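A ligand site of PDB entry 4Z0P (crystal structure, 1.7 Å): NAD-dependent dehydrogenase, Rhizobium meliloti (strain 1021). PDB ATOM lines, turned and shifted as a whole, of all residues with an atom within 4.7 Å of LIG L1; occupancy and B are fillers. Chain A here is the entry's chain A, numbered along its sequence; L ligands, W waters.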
ATOM      1  N   ALA A  75     -13.860 -17.726 -12.544  1.00  0.00           N
ATOM      2  CA  ALA A  75     -12.414 -17.518 -12.692  1.00  0.00           C
ATOM      3  C   ALA A  75     -11.964 -17.641 -14.118  1.00  0.00           C
ATOM      4  O   ALA A  75     -10.969 -17.019 -14.500  1.00  0.00           O
ATOM      5  CB  ALA A  75     -11.646 -18.500 -11.828  1.00  0.00           C
ATOM      6  N   GLY A  76     -12.657 -18.485 -14.870  1.00  0.00           N
ATOM      7  CA  GLY A  76     -12.319 -18.760 -16.265  1.00  0.00           C
ATOM      8  C   GLY A  76     -13.036 -17.772 -17.167  1.00  0.00           C
ATOM      9  O   GLY A  76     -14.137 -17.339 -16.860  1.00  0.00           O
ATOM     10  N   ASP A  78     -12.692 -18.130 -20.838  1.00  0.00           N
ATOM     11  CA  ASP A  78     -12.621 -18.638 -22.222  1.00  0.00           C
ATOM     12  C   ASP A  78     -13.938 -18.470 -22.988  1.00  0.00           C
ATOM     13  O   ASP A  78     -13.924 -18.163 -24.171  1.00  0.00           O
ATOM     14  CB  ASP A  78     -12.144 -20.070 -22.276  1.00  0.00           C
ATOM     15  CG  ASP A  78     -12.981 -21.008 -21.417  1.00  0.00           C
ATOM     16  OD1 ASP A  78     -13.020 -20.815 -20.175  1.00  0.00           O
ATOM     17  OD2 ASP A  78     -13.599 -21.913 -22.001  1.00  0.00           O
ATOM     18  N   ARG A  93     -11.765 -11.023 -13.963  1.00  0.00           N
ATOM     19  CA  ARG A  93     -12.200 -12.397 -13.615  1.00  0.00           C
ATOM     20  C   ARG A  93     -12.491 -12.494 -12.114  1.00  0.00           C
ATOM     21  O   ARG A  93     -12.073 -11.651 -11.329  1.00  0.00           O
ATOM     22  CB  ARG A  93     -11.150 -13.429 -14.065  1.00  0.00           C
ATOM     23  CG  ARG A  93      -9.915 -13.504 -13.180  1.00  0.00           C
ATOM     24  CD  ARG A  93      -8.755 -14.179 -13.884  1.00  0.00           C
ATOM     25  NE  ARG A  93      -7.698 -14.533 -12.954  1.00  0.00           N
ATOM     26  CZ  ARG A  93      -7.629 -15.690 -12.291  1.00  0.00           C
ATOM     27  NH1 ARG A  93      -8.551 -16.630 -12.443  1.00  0.00           N
ATOM     28  NH2 ARG A  93      -6.630 -15.886 -11.466  1.00  0.00           N
ATOM     29  N   LEU A  99     -14.011 -19.119  -3.707  1.00  0.00           N
ATOM     30  CA  LEU A  99     -13.830 -19.965  -4.891  1.00  0.00           C
ATOM     31  C   LEU A  99     -12.633 -20.896  -4.711  1.00  0.00           C
ATOM     32  O   LEU A  99     -12.692 -22.115  -4.953  1.00  0.00           O
ATOM     33  CB  LEU A  99     -13.680 -19.084  -6.140  1.00  0.00           C
ATOM     34  CG  LEU A  99     -13.769 -19.820  -7.479  1.00  0.00           C
ATOM     35  CD1 LEU A  99     -15.159 -20.310  -7.768  1.00  0.00           C
ATOM     36  CD2 LEU A  99     -13.368 -18.836  -8.580  1.00  0.00           C
ATOM     37  N   MET A 103     -12.519 -25.106  -4.607  1.00  0.00           N
ATOM     38  CA  MET A 103     -11.746 -25.931  -5.530  1.00  0.00           C
ATOM     39  C   MET A 103     -10.848 -26.899  -4.747  1.00  0.00           C
ATOM     40  O   MET A 103     -10.771 -28.095  -5.080  1.00  0.00           O
ATOM     41  CB  MET A 103     -10.915 -25.103  -6.484  1.00  0.00           C
ATOM     42  CG  MET A 103     -10.100 -25.928  -7.465  1.00  0.00           C
ATOM     43  SD  MET A 103     -11.081 -27.026  -8.497  1.00  0.00           S
ATOM     44  CE  MET A 103     -11.612 -25.901  -9.788  1.00  0.00           C
ATOM     45  N   GLY A 147      -0.837 -26.186 -13.796  1.00  0.00           N
ATOM     46  CA  GLY A 147      -1.477 -24.909 -13.490  1.00  0.00           C
ATOM     47  C   GLY A 147      -1.182 -24.511 -12.068  1.00  0.00           C
ATOM     48  O   GLY A 147      -1.737 -25.104 -11.147  1.00  0.00           O
ATOM     49  N   MET A 148      -0.294 -23.540 -11.889  1.00  0.00           N
ATOM     50  CA  MET A 148       0.205 -23.113 -10.569  1.00  0.00           C
ATOM     51  C   MET A 148      -0.245 -21.685 -10.297  1.00  0.00           C
ATOM     52  O   MET A 148       0.559 -20.834  -9.887  1.00  0.00           O
ATOM     53  CB  MET A 148       1.741 -23.164 -10.552  1.00  0.00           C
ATOM     54  CG  MET A 148       2.310 -24.548 -10.355  1.00  0.00           C
ATOM     55  SD  MET A 148       2.152 -25.039  -8.630  1.00  0.00           S
ATOM     56  CE  MET A 148       0.683 -26.046  -8.688  1.00  0.00           C
ATOM     57  N   GLY A 149      -1.511 -21.409 -10.539  1.00  0.00           N
ATOM     58  CA  GLY A 149      -2.080 -20.108 -10.315  1.00  0.00           C
ATOM     59  C   GLY A 149      -2.789 -20.049  -8.972  1.00  0.00           C
ATOM     60  O   GLY A 149      -2.411 -20.746  -8.022  1.00  0.00           O
ATOM     61  N   VAL A 150      -3.836 -19.249  -8.909  1.00  0.00           N
ATOM     62  CA  VAL A 150      -4.573 -19.095  -7.649  1.00  0.00           C
ATOM     63  C   VAL A 150      -5.050 -20.460  -7.153  1.00  0.00           C
ATOM     64  O   VAL A 150      -4.830 -20.834  -5.979  1.00  0.00           O
ATOM     65  CB  VAL A 150      -5.764 -18.129  -7.819  1.00  0.00           C
ATOM     66  CG1 VAL A 150      -6.628 -18.090  -6.564  1.00  0.00           C
ATOM     67  CG2 VAL A 150      -5.257 -16.718  -8.105  1.00  0.00           C
ATOM     68  N   LEU A 151      -5.661 -21.241  -8.036  1.00  0.00           N
ATOM     69  CA  LEU A 151      -6.266 -22.517  -7.626  1.00  0.00           C
ATOM     70  C   LEU A 151      -5.206 -23.594  -7.431  1.00  0.00           C
ATOM     71  O   LEU A 151      -5.198 -24.301  -6.412  1.00  0.00           O
ATOM     72  CB  LEU A 151      -7.354 -22.943  -8.619  1.00  0.00           C
ATOM     73  CG  LEU A 151      -8.500 -21.946  -8.764  1.00  0.00           C
ATOM     74  CD1 LEU A 151      -9.572 -22.450  -9.743  1.00  0.00           C
ATOM     75  CD2 LEU A 151      -9.132 -21.547  -7.438  1.00  0.00           C
ATOM     76  N   GLY A 152      -4.282 -23.710  -8.384  1.00  0.00           N
ATOM     77  CA  GLY A 152      -3.222 -24.704  -8.286  1.00  0.00           C
ATOM     78  C   GLY A 152      -2.360 -24.551  -7.048  1.00  0.00           C
ATOM     79  O   GLY A 152      -2.030 -25.547  -6.378  1.00  0.00           O
ATOM     80  N   TRP A 169       3.535 -27.709 -12.162  1.00  0.00           N
ATOM     81  CA  TRP A 169       4.023 -27.303 -13.477  1.00  0.00           C
ATOM     82  C   TRP A 169       3.214 -26.138 -13.991  1.00  0.00           C
ATOM     83  O   TRP A 169       1.986 -26.083 -13.824  1.00  0.00           O
ATOM     84  CB  TRP A 169       3.933 -28.480 -14.452  1.00  0.00           C
ATOM     85  CG  TRP A 169       4.345 -28.174 -15.851  1.00  0.00           C
ATOM     86  CD1 TRP A 169       5.597 -28.241 -16.377  1.00  0.00           C
ATOM     87  CD2 TRP A 169       3.482 -27.761 -16.930  1.00  0.00           C
ATOM     88  NE1 TRP A 169       5.592 -27.906 -17.709  1.00  0.00           N
ATOM     89  CE2 TRP A 169       4.304 -27.582 -18.066  1.00  0.00           C
ATOM     90  CE3 TRP A 169       2.115 -27.507 -17.045  1.00  0.00           C
ATOM     91  CZ2 TRP A 169       3.784 -27.211 -19.324  1.00  0.00           C
ATOM     92  CZ3 TRP A 169       1.596 -27.109 -18.282  1.00  0.00           C
ATOM     93  CH2 TRP A 169       2.430 -26.966 -19.401  1.00  0.00           C
ATOM     94  N   SER A 170       3.908 -25.190 -14.614  1.00  0.00           N
ATOM     95  CA  SER A 170       3.239 -24.082 -15.326  1.00  0.00           C
ATOM     96  C   SER A 170       4.224 -23.517 -16.307  1.00  0.00           C
ATOM     97  O   SER A 170       5.355 -24.010 -16.409  1.00  0.00           O
ATOM     98  CB  SER A 170       2.709 -23.036 -14.339  1.00  0.00           C
ATOM     99  OG  SER A 170       3.754 -22.525 -13.528  1.00  0.00           O
ATOM    100  N   ARG A 171       3.832 -22.473 -17.025  1.00  0.00           N
ATOM    101  CA  ARG A 171       4.702 -21.948 -18.081  1.00  0.00           C
ATOM    102  C   ARG A 171       5.986 -21.383 -17.508  1.00  0.00           C
ATOM    103  O   ARG A 171       7.088 -21.736 -17.953  1.00  0.00           O
ATOM    104  CB  ARG A 171       3.953 -20.929 -18.937  1.00  0.00           C
ATOM    105  CG  ARG A 171       4.777 -20.414 -20.107  1.00  0.00           C
ATOM    106  CD  ARG A 171       3.912 -20.156 -21.336  1.00  0.00           C
ATOM    107  NE  ARG A 171       2.744 -19.351 -21.030  1.00  0.00           N
ATOM    108  CZ  ARG A 171       1.745 -19.105 -21.873  1.00  0.00           C
ATOM    109  NH1 ARG A 171       1.763 -19.582 -23.126  1.00  0.00           N
ATOM    110  NH2 ARG A 171       0.725 -18.352 -21.472  1.00  0.00           N
ATOM    111  N   SER A 172       5.839 -20.493 -16.539  1.00  0.00           N
ATOM    112  CA  SER A 172       6.984 -19.992 -15.785  1.00  0.00           C
ATOM    113  C   SER A 172       7.072 -20.795 -14.489  1.00  0.00           C
ATOM    114  O   SER A 172       6.080 -21.330 -14.002  1.00  0.00           O
ATOM    115  CB  SER A 172       6.840 -18.493 -15.497  1.00  0.00           C
ATOM    116  OG  SER A 172       5.543 -18.155 -15.021  1.00  0.00           O
ATOM    117  N   ARG A 174       7.276 -21.271 -10.561  1.00  0.00           N
ATOM    118  CA  ARG A 174       6.738 -20.570  -9.397  1.00  0.00           C
ATOM    119  C   ARG A 174       7.467 -21.040  -8.137  1.00  0.00           C
ATOM    120  O   ARG A 174       7.784 -22.216  -8.021  1.00  0.00           O
ATOM    121  CB  ARG A 174       5.242 -20.881  -9.255  1.00  0.00           C
ATOM    122  CG  ARG A 174       4.370 -20.428 -10.423  1.00  0.00           C
ATOM    123  CD  ARG A 174       3.897 -18.979 -10.288  1.00  0.00           C
ATOM    124  NE  ARG A 174       2.668 -18.754 -11.055  1.00  0.00           N
ATOM    125  CZ  ARG A 174       1.838 -17.710 -10.893  1.00  0.00           C
ATOM    126  NH1 ARG A 174       0.742 -17.610 -11.657  1.00  0.00           N
ATOM    127  NH2 ARG A 174       2.067 -16.761  -9.971  1.00  0.00           N
ATOM    128  N   LEU A 200      -5.494 -27.928 -13.463  1.00  0.00           N
ATOM    129  CA  LEU A 200      -6.069 -26.645 -13.057  1.00  0.00           C
ATOM    130  C   LEU A 200      -5.563 -25.523 -13.965  1.00  0.00           C
ATOM    131  O   LEU A 200      -5.171 -24.463 -13.510  1.00  0.00           O
ATOM    132  CB  LEU A 200      -5.739 -26.353 -11.605  1.00  0.00           C
ATOM    133  CG  LEU A 200      -6.571 -27.205 -10.622  1.00  0.00           C
ATOM    134  CD1 LEU A 200      -5.997 -27.083  -9.217  1.00  0.00           C
ATOM    135  CD2 LEU A 200      -8.027 -26.828 -10.645  1.00  0.00           C
ATOM    136  N   LEU A 201      -5.597 -25.803 -15.260  1.00  0.00           N
ATOM    137  CA  LEU A 201      -5.214 -24.853 -16.310  1.00  0.00           C
ATOM    138  C   LEU A 201      -6.463 -24.173 -16.869  1.00  0.00           C
ATOM    139  O   LEU A 201      -7.530 -24.773 -16.941  1.00  0.00           O
ATOM    140  CB  LEU A 201      -4.545 -25.572 -17.474  1.00  0.00           C
ATOM    141  CG  LEU A 201      -3.130 -26.147 -17.271  1.00  0.00           C
ATOM    142  CD1 LEU A 201      -2.783 -27.091 -18.406  1.00  0.00           C
ATOM    143  CD2 LEU A 201      -2.111 -25.029 -17.136  1.00  0.00           C
ATOM    144  N   PRO A 202      -6.334 -22.915 -17.305  1.00  0.00           N
ATOM    145  CA  PRO A 202      -7.364 -22.315 -18.167  1.00  0.00           C
ATOM    146  C   PRO A 202      -7.408 -23.025 -19.522  1.00  0.00           C
ATOM    147  O   PRO A 202      -6.436 -23.707 -19.872  1.00  0.00           O
ATOM    148  CB  PRO A 202      -6.921 -20.866 -18.330  1.00  0.00           C
ATOM    149  CG  PRO A 202      -5.466 -20.858 -17.973  1.00  0.00           C
ATOM    150  CD  PRO A 202      -5.093 -22.110 -17.251  1.00  0.00           C
ATOM    151  N   LEU A 203      -8.533 -22.882 -20.218  1.00  0.00           N
ATOM    152  CA  LEU A 203      -8.604 -23.207 -21.642  1.00  0.00           C
ATOM    153  C   LEU A 203      -8.105 -22.016 -22.414  1.00  0.00           C
ATOM    154  O   LEU A 203      -8.683 -20.927 -22.320  1.00  0.00           O
ATOM    155  CB  LEU A 203     -10.015 -23.538 -22.122  1.00  0.00           C
ATOM    156  CG  LEU A 203     -10.120 -23.946 -23.616  1.00  0.00           C
ATOM    157  CD1 LEU A 203      -9.239 -25.116 -23.984  1.00  0.00           C
ATOM    158  CD2 LEU A 203     -11.558 -24.244 -23.979  1.00  0.00           C
ATOM    159  N   ASP A 206      -3.362 -22.494 -26.486  1.00  0.00           N
ATOM    160  CA  ASP A 206      -2.177 -23.257 -26.153  1.00  0.00           C
ATOM    161  C   ASP A 206      -2.444 -24.448 -25.225  1.00  0.00           C
ATOM    162  O   ASP A 206      -1.610 -25.329 -25.137  1.00  0.00           O
ATOM    163  CB  ASP A 206      -1.099 -22.356 -25.521  1.00  0.00           C
ATOM    164  CG  ASP A 206      -0.480 -21.400 -26.486  1.00  0.00           C
ATOM    165  OD1 ASP A 206      -0.519 -21.643 -27.697  1.00  0.00           O
ATOM    166  OD2 ASP A 206       0.045 -20.388 -26.024  1.00  0.00           O
ATOM    167  N   THR A 207      -3.567 -24.488 -24.522  1.00  0.00           N
ATOM    168  CA  THR A 207      -3.888 -25.650 -23.655  1.00  0.00           C
ATOM    169  C   THR A 207      -4.948 -26.552 -24.259  1.00  0.00           C
ATOM    170  O   THR A 207      -5.358 -27.543 -23.634  1.00  0.00           O
ATOM    171  CB  THR A 207      -4.322 -25.241 -22.248  1.00  0.00           C
ATOM    172  OG1 THR A 207      -5.635 -24.656 -22.255  1.00  0.00           O
ATOM    173  CG2 THR A 207      -3.346 -24.277 -21.597  1.00  0.00           C
ATOM    174  N   ALA A 233     -10.217 -30.448 -13.371  1.00  0.00           N
ATOM    175  CA  ALA A 233     -11.239 -29.450 -13.039  1.00  0.00           C
ATOM    176  C   ALA A 233     -10.935 -28.092 -13.640  1.00  0.00           C
ATOM    177  O   ALA A 233     -11.487 -27.073 -13.179  1.00  0.00           O
ATOM    178  CB  ALA A 233     -11.425 -29.334 -11.534  1.00  0.00           C
ATOM    179  N   GLY A 234     -10.130 -28.076 -14.690  1.00  0.00           N
ATOM    180  CA  GLY A 234      -9.852 -26.853 -15.435  1.00  0.00           C
ATOM    181  C   GLY A 234     -10.936 -26.602 -16.457  1.00  0.00           C
ATOM    182  O   GLY A 234     -12.004 -26.025 -16.138  1.00  0.00           O
ATOM    183  N   ARG A 235     -10.687 -27.050 -17.684  1.00  0.00           N
ATOM    184  CA  ARG A 235     -11.695 -26.983 -18.737  1.00  0.00           C
ATOM    185  C   ARG A 235     -11.657 -28.230 -19.574  1.00  0.00           C
ATOM    186  O   ARG A 235     -10.599 -28.805 -19.820  1.00  0.00           O
ATOM    187  CB  ARG A 235     -11.412 -25.778 -19.646  1.00  0.00           C
ATOM    188  CG  ARG A 235     -11.759 -24.434 -19.030  1.00  0.00           C
ATOM    189  CD  ARG A 235     -13.256 -24.255 -19.006  1.00  0.00           C
ATOM    190  NE  ARG A 235     -13.703 -23.001 -18.439  1.00  0.00           N
ATOM    191  CZ  ARG A 235     -13.984 -22.785 -17.167  1.00  0.00           C
ATOM    192  NH1 ARG A 235     -13.819 -23.738 -16.246  1.00  0.00           N
ATOM    193  NH2 ARG A 235     -14.422 -21.596 -16.807  1.00  0.00           N
ATOM    194  N   ASP A 259     -14.542 -33.244 -13.781  1.00  0.00           N
ATOM    195  CA  ASP A 259     -15.564 -32.236 -13.489  1.00  0.00           C
ATOM    196  C   ASP A 259     -15.965 -31.452 -14.725  1.00  0.00           C
ATOM    197  O   ASP A 259     -16.954 -30.717 -14.695  1.00  0.00           O
ATOM    198  CB  ASP A 259     -15.041 -31.236 -12.449  1.00  0.00           C
ATOM    199  CG  ASP A 259     -16.145 -30.335 -11.906  1.00  0.00           C
ATOM    200  OD1 ASP A 259     -17.192 -30.848 -11.389  1.00  0.00           O
ATOM    201  OD2 ASP A 259     -15.959 -29.094 -11.987  1.00  0.00           O
ATOM    202  N   VAL A 260     -15.150 -31.563 -15.783  1.00  0.00           N
ATOM    203  CA  VAL A 260     -15.278 -30.719 -16.989  1.00  0.00           C
ATOM    204  C   VAL A 260     -15.137 -31.601 -18.220  1.00  0.00           C
ATOM    205  O   VAL A 260     -14.448 -32.626 -18.166  1.00  0.00           O
ATOM    206  CB  VAL A 260     -14.261 -29.558 -16.983  1.00  0.00           C
ATOM    207  CG1 VAL A 260     -14.532 -28.624 -15.821  1.00  0.00           C
ATOM    208  CG2 VAL A 260     -12.834 -30.089 -16.911  1.00  0.00           C
ATOM    209  N   HIS A 283     -19.505 -30.060 -13.518  1.00  0.00           N
ATOM    210  CA  HIS A 283     -18.856 -28.756 -13.497  1.00  0.00           C
ATOM    211  C   HIS A 283     -19.239 -27.957 -12.252  1.00  0.00           C
ATOM    212  O   HIS A 283     -19.771 -26.842 -12.306  1.00  0.00           O
ATOM    213  CB  HIS A 283     -19.133 -28.003 -14.785  1.00  0.00           C
ATOM    214  CG  HIS A 283     -18.196 -26.861 -15.031  1.00  0.00           C
ATOM    215  ND1 HIS A 283     -17.874 -26.442 -16.299  1.00  0.00           N
ATOM    216  CD2 HIS A 283     -17.523 -26.045 -14.187  1.00  0.00           C
ATOM    217  CE1 HIS A 283     -17.052 -25.412 -16.228  1.00  0.00           C
ATOM    218  NE2 HIS A 283     -16.820 -25.158 -14.965  1.00  0.00           N
ATOM    219  N   VAL A 284     -18.975 -28.595 -11.119  1.00  0.00           N
ATOM    220  CA  VAL A 284     -19.262 -28.078  -9.781  1.00  0.00           C
ATOM    221  C   VAL A 284     -18.041 -28.087  -8.850  1.00  0.00           C
ATOM    222  O   VAL A 284     -18.166 -27.992  -7.619  1.00  0.00           O
ATOM    223  CB  VAL A 284     -20.439 -28.851  -9.124  1.00  0.00           C
ATOM    224  CG1 VAL A 284     -21.756 -28.503  -9.790  1.00  0.00           C
ATOM    225  CG2 VAL A 284     -20.203 -30.376  -9.113  1.00  0.00           C
ATOM    226  N   ALA A 285     -16.817 -28.184  -9.394  1.00  0.00           N
ATOM    227  CA  ALA A 285     -15.657 -28.314  -8.510  1.00  0.00           C
ATOM    228  C   ALA A 285     -15.541 -27.074  -7.607  1.00  0.00           C
ATOM    229  O   ALA A 285     -15.274 -27.211  -6.420  1.00  0.00           O
ATOM    230  CB  ALA A 285     -14.374 -28.535  -9.293  1.00  0.00           C
ATOM    231  N   ALA A 286     -15.792 -25.887  -8.169  1.00  0.00           N
ATOM    232  CA  ALA A 286     -15.813 -24.681  -7.337  1.00  0.00           C
ATOM    233  C   ALA A 286     -16.916 -23.776  -7.808  1.00  0.00           C
ATOM    234  O   ALA A 286     -16.765 -23.058  -8.811  1.00  0.00           O
ATOM    235  CB  ALA A 286     -14.470 -23.983  -7.375  1.00  0.00           C
ATOM    236  N   TYR A 320      -6.339 -15.471 -20.524  1.00  0.00           N
ATOM    237  CA  TYR A 320      -6.504 -15.691 -19.069  1.00  0.00           C
ATOM    238  C   TYR A 320      -5.863 -14.576 -18.276  1.00  0.00           C
ATOM    239  O   TYR A 320      -5.190 -13.711 -18.838  1.00  0.00           O
ATOM    240  CB  TYR A 320      -5.956 -17.062 -18.634  1.00  0.00           C
ATOM    241  CG  TYR A 320      -4.475 -17.214 -18.654  1.00  0.00           C
ATOM    242  CD1 TYR A 320      -3.799 -17.418 -19.866  1.00  0.00           C
ATOM    243  CD2 TYR A 320      -3.712 -17.156 -17.495  1.00  0.00           C
ATOM    244  CE1 TYR A 320      -2.426 -17.585 -19.900  1.00  0.00           C
ATOM    245  CE2 TYR A 320      -2.328 -17.293 -17.539  1.00  0.00           C
ATOM    246  CZ  TYR A 320      -1.693 -17.514 -18.746  1.00  0.00           C
ATOM    247  OH  TYR A 320      -0.336 -17.672 -18.828  1.00  0.00           O
ATOM    248  OXT TYR A 320      -6.010 -14.582 -17.046  1.00  0.00           O
HETATM  249  P1  LIG L   1      -4.698 -18.517 -12.822  1.00  0.00           P
HETATM  250  O1  LIG L   1      -4.657 -17.550 -13.988  1.00  0.00           O
HETATM  251  O2  LIG L   1      -4.431 -17.969 -11.459  1.00  0.00           O
HETATM  252  O3  LIG L   1      -3.633 -19.642 -13.137  1.00  0.00           O
HETATM  253  C1  LIG L   1      -3.465 -20.235 -14.409  1.00  0.00           C
HETATM  254  C2  LIG L   1      -2.207 -21.060 -14.375  1.00  0.00           C
HETATM  255  O4  LIG L   1      -2.137 -21.777 -15.606  1.00  0.00           O
HETATM  256  C3  LIG L   1      -0.917 -20.239 -14.277  1.00  0.00           C
HETATM  257  O5  LIG L   1      -0.006 -20.967 -13.463  1.00  0.00           O
HETATM  258  C4  LIG L   1      -0.432 -20.196 -15.710  1.00  0.00           C
HETATM  259  O6  LIG L   1       0.966 -20.054 -15.875  1.00  0.00           O
HETATM  260  C5  LIG L   1      -0.857 -21.570 -16.175  1.00  0.00           C
HETATM  261  N1  LIG L   1      -0.900 -21.620 -17.641  1.00  0.00           N
HETATM  262  C6  LIG L   1      -1.720 -20.989 -18.514  1.00  0.00           C
HETATM  263  N2  LIG L   1      -1.468 -21.272 -19.774  1.00  0.00           N
HETATM  264  C7  LIG L   1      -0.410 -22.135 -19.710  1.00  0.00           C
HETATM  265  C8  LIG L   1       0.352 -22.786 -20.704  1.00  0.00           C
HETATM  266  N3  LIG L   1       0.093 -22.655 -22.025  1.00  0.00           N
HETATM  267  N4  LIG L   1       1.373 -23.602 -20.297  1.00  0.00           N
HETATM  268  C9  LIG L   1       1.614 -23.733 -18.994  1.00  0.00           C
HETATM  269  N5  LIG L   1       0.971 -23.153 -17.971  1.00  0.00           N
HETATM  270  C10 LIG L   1      -0.051 -22.365 -18.399  1.00  0.00           C
HETATM  271  O7  LIG L   1      -6.144 -19.234 -12.951  1.00  0.00           O
HETATM  272  P2  LIG L   1      -6.905 -19.899 -11.686  1.00  0.00           P
HETATM  273  O8  LIG L   1      -5.966 -20.771 -10.915  1.00  0.00           O
HETATM  274  O9  LIG L   1      -7.688 -18.871 -10.955  1.00  0.00           O
HETATM  275  O10 LIG L   1      -7.981 -20.740 -12.498  1.00  0.00           O
HETATM  276  C11 LIG L   1      -7.544 -21.786 -13.348  1.00  0.00           C
HETATM  277  C12 LIG L   1      -8.695 -22.303 -14.194  1.00  0.00           C
HETATM  278  O11 LIG L   1      -9.561 -23.131 -13.417  1.00  0.00           O
HETATM  279  C13 LIG L   1      -9.659 -21.261 -14.761  1.00  0.00           C
HETATM  280  O12 LIG L   1      -9.103 -20.638 -15.934  1.00  0.00           O
HETATM  281  C14 LIG L   1     -10.929 -22.025 -15.072  1.00  0.00           C
HETATM  282  O13 LIG L   1     -10.905 -22.517 -16.427  1.00  0.00           O
HETATM  283  C15 LIG L   1     -10.807 -23.225 -14.095  1.00  0.00           C
HETATM  284  N6  LIG L   1     -11.885 -23.265 -13.104  1.00  0.00           N
HETATM  285  C16 LIG L   1     -12.781 -24.328 -13.064  1.00  0.00           C
HETATM  286  C17 LIG L   1     -13.776 -24.392 -12.148  1.00  0.00           C
HETATM  287  C18 LIG L   1     -14.663 -25.597 -11.984  1.00  0.00           C
HETATM  288  O14 LIG L   1     -15.705 -25.458 -11.315  1.00  0.00           O
HETATM  289  N7  LIG L   1     -14.339 -26.732 -12.547  1.00  0.00           N
HETATM  290  C19 LIG L   1     -13.956 -23.277 -11.184  1.00  0.00           C
HETATM  291  C20 LIG L   1     -12.975 -22.174 -11.307  1.00  0.00           C
HETATM  292  C21 LIG L   1     -11.990 -22.205 -12.195  1.00  0.00           C
HETATM  293  P3  LIG L   1       1.698 -18.654 -15.589  1.00  0.00           P
HETATM  294  O15 LIG L   1       1.660 -18.519 -14.097  1.00  0.00           O
HETATM  295  O16 LIG L   1       3.093 -18.923 -16.138  1.00  0.00           O
HETATM  296  O17 LIG L   1       0.939 -17.615 -16.321  1.00  0.00           O
HETATM  297  C1  LG2 L   2     -15.210 -20.822 -13.279  1.00  0.00           C
HETATM  298  C2  LG2 L   2     -16.034 -21.997 -13.529  1.00  0.00           C
HETATM  299  O1  LG2 L   2     -15.310 -20.198 -12.199  1.00  0.00           O
HETATM  300  O2  LG2 L   2     -17.160 -22.076 -13.009  1.00  0.00           O
HETATM  301  O3  LG2 L   2     -14.418 -20.467 -14.189  1.00  0.00           O
HETATM  302  O4  LG2 L   2     -15.612 -22.902 -14.258  1.00  0.00           O
HETATM  303  O   HOH W   1      -8.911 -17.956 -16.129  1.00  0.00           O
HETATM  304  O   HOH W   2     -18.346 -24.582 -10.934  1.00  0.00           O
HETATM  305  O   HOH W   3      -2.006 -20.654 -22.446  1.00  0.00           O
HETATM  306  O   HOH W   4      -3.170 -15.352 -14.099  1.00  0.00           O
HETATM  307  O   HOH W   5      -4.118 -22.741 -11.212  1.00  0.00           O
HETATM  308  O   HOH W   6      -0.452 -16.540 -14.152  1.00  0.00           O
HETATM  309  O   HOH W   7      -2.317 -16.393 -10.960  1.00  0.00           O
HETATM  310  O   HOH W   8      -9.571 -17.740  -9.151  1.00  0.00           O
HETATM  311  O   HOH W   9       3.524 -17.607 -18.718  1.00  0.00           O
HETATM  312  O   HOH W  10     -10.514 -21.073 -18.833  1.00  0.00           O
HETATM  313  O   HOH W  11      -6.860 -16.520 -15.281  1.00  0.00           O
HETATM  314  O   HOH W  12       3.573 -24.247 -21.874  1.00  0.00           O
HETATM  315  O   HOH W  13       1.828 -23.705 -24.176  1.00  0.00           O
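Water W7 lies within hydrogen-bond range of an oxygen (O2) of LIG L1 (2.7 Å) and the guanidinium group of Arg 174 (3.4 Å). Water W1 bridges an oxygen (O12) of LIG L1 and the backbone carbonyl oxygen (O) of Ala 75. Water W11 lies within hydrogen-bond range of an oxygen (O1) of LIG L1 (2.8 Å), the chain-end carboxylate (OXT) of Tyr 320 (2.8 Å) and the guanidinium group (NE) of Arg 93 (3.2 Å). Water W6 bridges O17 of LIG L1 and NH1 of Arg 174. Water W10 lies within hydrogen-bond range of O13 of LIG L1 (2.8 Å), OD1 of Asp 78 (2.9 Å) and N of Leu 203 (3.0 Å). Water W9 bridges an oxygen (O16) of LIG L1 (2.9 Å) and the guanidinium group (NE) of Arg 171 (3.0 Å).
CB of Ala 75 touches C21 of LIG L1, at 3.7 Å. Gly 76 touches LIG L1. Met 103 touches LIG L1. Gly 147 touches LIG L1. CH2 of Trp 169 touches C9 of LIG L1, 3.4 Å away. Ser 170 touches LIG L1 (CB to O5, 3.5 Å). Leu 200 touches LIG L1. Leu 201 touches LIG L1 (CD2 to O4, 3.6 Å). Pro 202 touches LIG L1. Asp 206 touches LIG L1. Thr 207 touches LIG L1 (CG2 to N3, 3.8 Å). O of Gly 234 touches C16 of LIG L1, 3.6 Å away. CG1 of Val 260 touches N7 of LIG L1, at 3.8 Å. His 283 touches LIG L1. Ala 285 touches LIG L1 (N to O14, 3.5 Å).
The backbone carbonyl oxygen (O) of Met 148 lies within hydrogen-bond range of the guanidinium group (NE) of Arg 174, 3.2 Å away. OG of Ser 170 is in hydrogen-bond range of O of Ser 172 (2.7 Å). The guanidinium group (NH2) of Arg 171 lies within hydrogen-bond range of the side-chain hydroxyl (OH) of Tyr 320, 2.9 Å away. NH1 of Arg 93 sits at hydrogen-bond distance from O of Ala 75 (3.2 Å). The side-chain carboxylate (OD2) of Asp 206 is in salt-bridge range of the guanidinium group (NH1) of Arg 171 (3.5 Å). The guanidinium group (NE) of Arg 235 lies within salt-bridge range of the side-chain carboxylate (OD1) of Asp 78, 2.9 Å away. O of Pro 202 is in hydrogen-bond range of OG1 of Thr 207, 2.7 Å away. The backbone carbonyl oxygen of Trp 169 lies within hydrogen-bond range of the backbone NH of Gly 147 (2.8 Å).
NH1 of Arg 174 lies within salt-bridge range of O15 of LIG L1 (2.8 Å). The backbone NH of Ser 172 is in hydrogen-bond range of an oxygen (O16) of LIG L1 (3.2 Å). O16 of LIG L1 is in hydrogen-bond range of OG of Ser 172 (2.8 Å). OH of Tyr 320 lies within hydrogen-bond range of O17 of LIG L1, 2.8 Å away. An oxygen (O9) of LIG L1 is in salt-bridge range of the guanidinium group (NH1) of Arg 93. N of Val 150 lies within hydrogen-bond range of O2 of LIG L1 (2.9 Å). OD2 of Asp 259 is in hydrogen-bond range of N7 of LIG L1. N of Leu 151 is in hydrogen-bond range of O8 of LIG L1 (2.9 Å). A nitrogen (N7) of LIG L1 lies within hydrogen-bond range of the backbone carbonyl oxygen of Ala 233 (2.9 Å). N of Met 148 sits at hydrogen-bond distance from O5 of LIG L1, 3.0 Å away. The backbone NH of Arg 171 sits at hydrogen-bond distance from a nitrogen (N5) of LIG L1 (3.1 Å). The guanidinium group of Arg 235 sits at hydrogen-bond distance from an oxygen (O13) of LIG L1, 3.2 Å away. N of Ala 286 sits at hydrogen-bond distance from O14 of LIG L1 (3.2 Å). An oxygen (O5) of LIG L1 is in hydrogen-bond range of the backbone NH of Gly 149 (3.3 Å). An oxygen (O4) of LG2 L2 lies within salt-bridge range of the guanidinium group of Arg 235, at 2.8 Å. A ring nitrogen (NE2) of His 283 lies within hydrogen-bond range of an oxygen (O4) of LG2 L2 (2.7 Å). The backbone NH (N) of Ala 75 is in hydrogen-bond range of an oxygen (O1) of LG2 L2. N of Gly 76 is in hydrogen-bond range of O3 of LG2 L2 (2.7 Å).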
